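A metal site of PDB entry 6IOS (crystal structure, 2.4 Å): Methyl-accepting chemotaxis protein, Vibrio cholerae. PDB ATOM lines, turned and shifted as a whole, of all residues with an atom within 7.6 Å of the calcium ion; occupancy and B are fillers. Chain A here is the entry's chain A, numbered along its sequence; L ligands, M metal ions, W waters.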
ATOM      1  N   GLU A  62       7.395  25.316  -3.644  1.00  0.00           N
ATOM      2  CA  GLU A  62       6.956  24.133  -2.897  1.00  0.00           C
ATOM      3  C   GLU A  62       7.417  24.129  -1.420  1.00  0.00           C
ATOM      4  O   GLU A  62       7.056  23.233  -0.664  1.00  0.00           O
ATOM      5  CB  GLU A  62       7.431  22.836  -3.601  1.00  0.00           C
ATOM      6  CG  GLU A  62       6.902  22.643  -5.040  1.00  0.00           C
ATOM      7  CD  GLU A  62       5.363  22.441  -5.167  1.00  0.00           C
ATOM      8  OE1 GLU A  62       4.680  22.111  -4.171  1.00  0.00           O
ATOM      9  OE2 GLU A  62       4.840  22.605  -6.290  1.00  0.00           O
ATOM     10  N   VAL A  84       5.418  28.510 -14.143  1.00  0.00           N
ATOM     11  CA  VAL A  84       5.876  27.683 -13.020  1.00  0.00           C
ATOM     12  C   VAL A  84       4.891  27.898 -11.881  1.00  0.00           C
ATOM     13  O   VAL A  84       4.584  29.047 -11.537  1.00  0.00           O
ATOM     14  CB  VAL A  84       7.294  28.049 -12.542  1.00  0.00           C
ATOM     15  CG1 VAL A  84       7.613  27.335 -11.239  1.00  0.00           C
ATOM     16  CG2 VAL A  84       8.344  27.724 -13.607  1.00  0.00           C
ATOM     17  N   GLU A  85       4.410  26.825 -11.283  1.00  0.00           N
ATOM     18  CA  GLU A  85       3.224  26.988 -10.459  1.00  0.00           C
ATOM     19  C   GLU A  85       3.059  25.868  -9.409  1.00  0.00           C
ATOM     20  O   GLU A  85       3.363  24.719  -9.689  1.00  0.00           O
ATOM     21  CB  GLU A  85       2.031  27.112 -11.440  1.00  0.00           C
ATOM     22  CG  GLU A  85       0.795  26.454 -11.041  1.00  0.00           C
ATOM     23  CD  GLU A  85       0.820  24.942 -11.164  1.00  0.00           C
ATOM     24  OE1 GLU A  85       1.498  24.342 -12.042  1.00  0.00           O
ATOM     25  OE2 GLU A  85       0.162  24.370 -10.315  1.00  0.00           O
ATOM     26  N   ASN A  86       2.588  26.209  -8.197  1.00  0.00           N
ATOM     27  CA  ASN A  86       2.544  25.234  -7.101  1.00  0.00           C
ATOM     28  C   ASN A  86       1.144  24.728  -6.751  1.00  0.00           C
ATOM     29  O   ASN A  86       0.907  24.241  -5.648  1.00  0.00           O
ATOM     30  CB  ASN A  86       3.187  25.807  -5.816  1.00  0.00           C
ATOM     31  CG  ASN A  86       2.308  26.899  -5.134  1.00  0.00           C
ATOM     32  OD1 ASN A  86       1.260  27.263  -5.633  1.00  0.00           O
ATOM     33  ND2 ASN A  86       2.767  27.401  -4.010  1.00  0.00           N
ATOM     34  N   ASP A  87       0.208  24.879  -7.693  1.00  0.00           N
ATOM     35  CA  ASP A  87      -1.157  24.430  -7.499  1.00  0.00           C
ATOM     36  C   ASP A  87      -1.233  22.922  -7.759  1.00  0.00           C
ATOM     37  O   ASP A  87      -1.050  22.472  -8.880  1.00  0.00           O
ATOM     38  CB  ASP A  87      -2.101  25.219  -8.422  1.00  0.00           C
ATOM     39  CG  ASP A  87      -3.563  24.957  -8.175  1.00  0.00           C
ATOM     40  OD1 ASP A  87      -3.967  23.861  -7.693  1.00  0.00           O
ATOM     41  OD2 ASP A  87      -4.378  25.857  -8.469  1.00  0.00           O
ATOM     42  N   ASP A  88      -1.522  22.144  -6.719  1.00  0.00           N
ATOM     43  CA  ASP A  88      -1.543  20.677  -6.845  1.00  0.00           C
ATOM     44  C   ASP A  88      -2.701  20.123  -7.680  1.00  0.00           C
ATOM     45  O   ASP A  88      -2.663  18.970  -8.094  1.00  0.00           O
ATOM     46  CB  ASP A  88      -1.565  20.013  -5.462  1.00  0.00           C
ATOM     47  CG  ASP A  88      -0.330  20.321  -4.658  1.00  0.00           C
ATOM     48  OD1 ASP A  88       0.780  20.010  -5.134  1.00  0.00           O
ATOM     49  OD2 ASP A  88      -0.453  20.888  -3.556  1.00  0.00           O
ATOM     50  N   GLY A  89      -3.746  20.911  -7.917  1.00  0.00           N
ATOM     51  CA  GLY A  89      -4.865  20.437  -8.701  1.00  0.00           C
ATOM     52  C   GLY A  89      -5.094  21.234  -9.980  1.00  0.00           C
ATOM     53  O   GLY A  89      -6.199  21.250 -10.503  1.00  0.00           O
ATOM     54  N   TRP A  90      -4.064  21.895 -10.482  1.00  0.00           N
ATOM     55  CA  TRP A  90      -4.207  22.666 -11.711  1.00  0.00           C
ATOM     56  C   TRP A  90      -2.956  22.716 -12.587  1.00  0.00           C
ATOM     57  O   TRP A  90      -1.829  22.943 -12.103  1.00  0.00           O
ATOM     58  CB  TRP A  90      -4.632  24.107 -11.416  1.00  0.00           C
ATOM     59  CG  TRP A  90      -4.861  24.879 -12.694  1.00  0.00           C
ATOM     60  CD1 TRP A  90      -5.971  24.838 -13.487  1.00  0.00           C
ATOM     61  CD2 TRP A  90      -3.951  25.789 -13.337  1.00  0.00           C
ATOM     62  NE1 TRP A  90      -5.810  25.658 -14.571  1.00  0.00           N
ATOM     63  CE2 TRP A  90      -4.580  26.262 -14.509  1.00  0.00           C
ATOM     64  CE3 TRP A  90      -2.678  26.277 -13.017  1.00  0.00           C
ATOM     65  CZ2 TRP A  90      -3.988  27.185 -15.359  1.00  0.00           C
ATOM     66  CZ3 TRP A  90      -2.081  27.184 -13.867  1.00  0.00           C
ATOM     67  CH2 TRP A  90      -2.746  27.632 -15.028  1.00  0.00           C
ATOM     68  N   GLU A  91      -3.168  22.526 -13.885  1.00  0.00           N
ATOM     69  CA  GLU A  91      -2.123  22.725 -14.874  1.00  0.00           C
ATOM     70  C   GLU A  91      -2.697  23.547 -16.007  1.00  0.00           C
ATOM     71  O   GLU A  91      -3.876  23.410 -16.347  1.00  0.00           O
ATOM     72  CB  GLU A  91      -1.577  21.382 -15.392  1.00  0.00           C
ATOM     73  CG  GLU A  91      -0.734  20.634 -14.379  1.00  0.00           C
ATOM     74  CD  GLU A  91       0.545  21.372 -14.037  1.00  0.00           C
ATOM     75  OE1 GLU A  91       0.961  21.378 -12.876  1.00  0.00           O
ATOM     76  OE2 GLU A  91       1.160  21.977 -14.945  1.00  0.00           O
ATOM     77  N   PRO A  92      -1.871  24.428 -16.590  1.00  0.00           N
ATOM     78  CA  PRO A  92      -2.306  25.157 -17.783  1.00  0.00           C
ATOM     79  C   PRO A  92      -2.452  24.220 -18.983  1.00  0.00           C
ATOM     80  O   PRO A  92      -1.861  23.124 -18.971  1.00  0.00           O
ATOM     81  CB  PRO A  92      -1.167  26.156 -18.023  1.00  0.00           C
ATOM     82  CG  PRO A  92       0.037  25.437 -17.500  1.00  0.00           C
ATOM     83  CD  PRO A  92      -0.442  24.661 -16.289  1.00  0.00           C
HETATM   84  C1  LIG L   1      -0.531  19.330 -10.372  1.00  0.00           C
HETATM   85  O1  LIG L   1      -1.548  19.992 -10.669  1.00  0.00           O
HETATM   86  O2  LIG L   1      -0.632  18.068 -10.336  1.00  0.00           O
HETATM   87  C2  LIG L   1       0.742  20.013 -10.064  1.00  0.00           C
HETATM   88 CA    CA M   1       0.131  22.297 -10.880  1.00  0.00          CA
HETATM   89  O   HOH W   1       2.182  22.617  -9.498  1.00  0.00           O
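The backbone NH of Trp 90 lies within hydrogen-bond range of the side-chain carboxylate of Asp 87.
The side-chain carboxylate (OD1) of Asp 87 is in hydrogen-bond range of the backbone NH (N) of Gly 89.
Within 4 Å of the calcium ion: Glu 85, Asp 87, Trp 90 and Glu 91.
The calcium ion is bound by OE2 of Glu 85 (2.1 Å), O of Asp 87 (2.3 Å), OE1 of Glu 91 (2.3 Å), O of Trp 90 (2.4 Å), water W1 (2.5 Å), OE1 of Glu 85 (2.7 Å) and O1 of the ligand (2.9 Å).
The calcium ion has seven donor atoms within binding distance.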
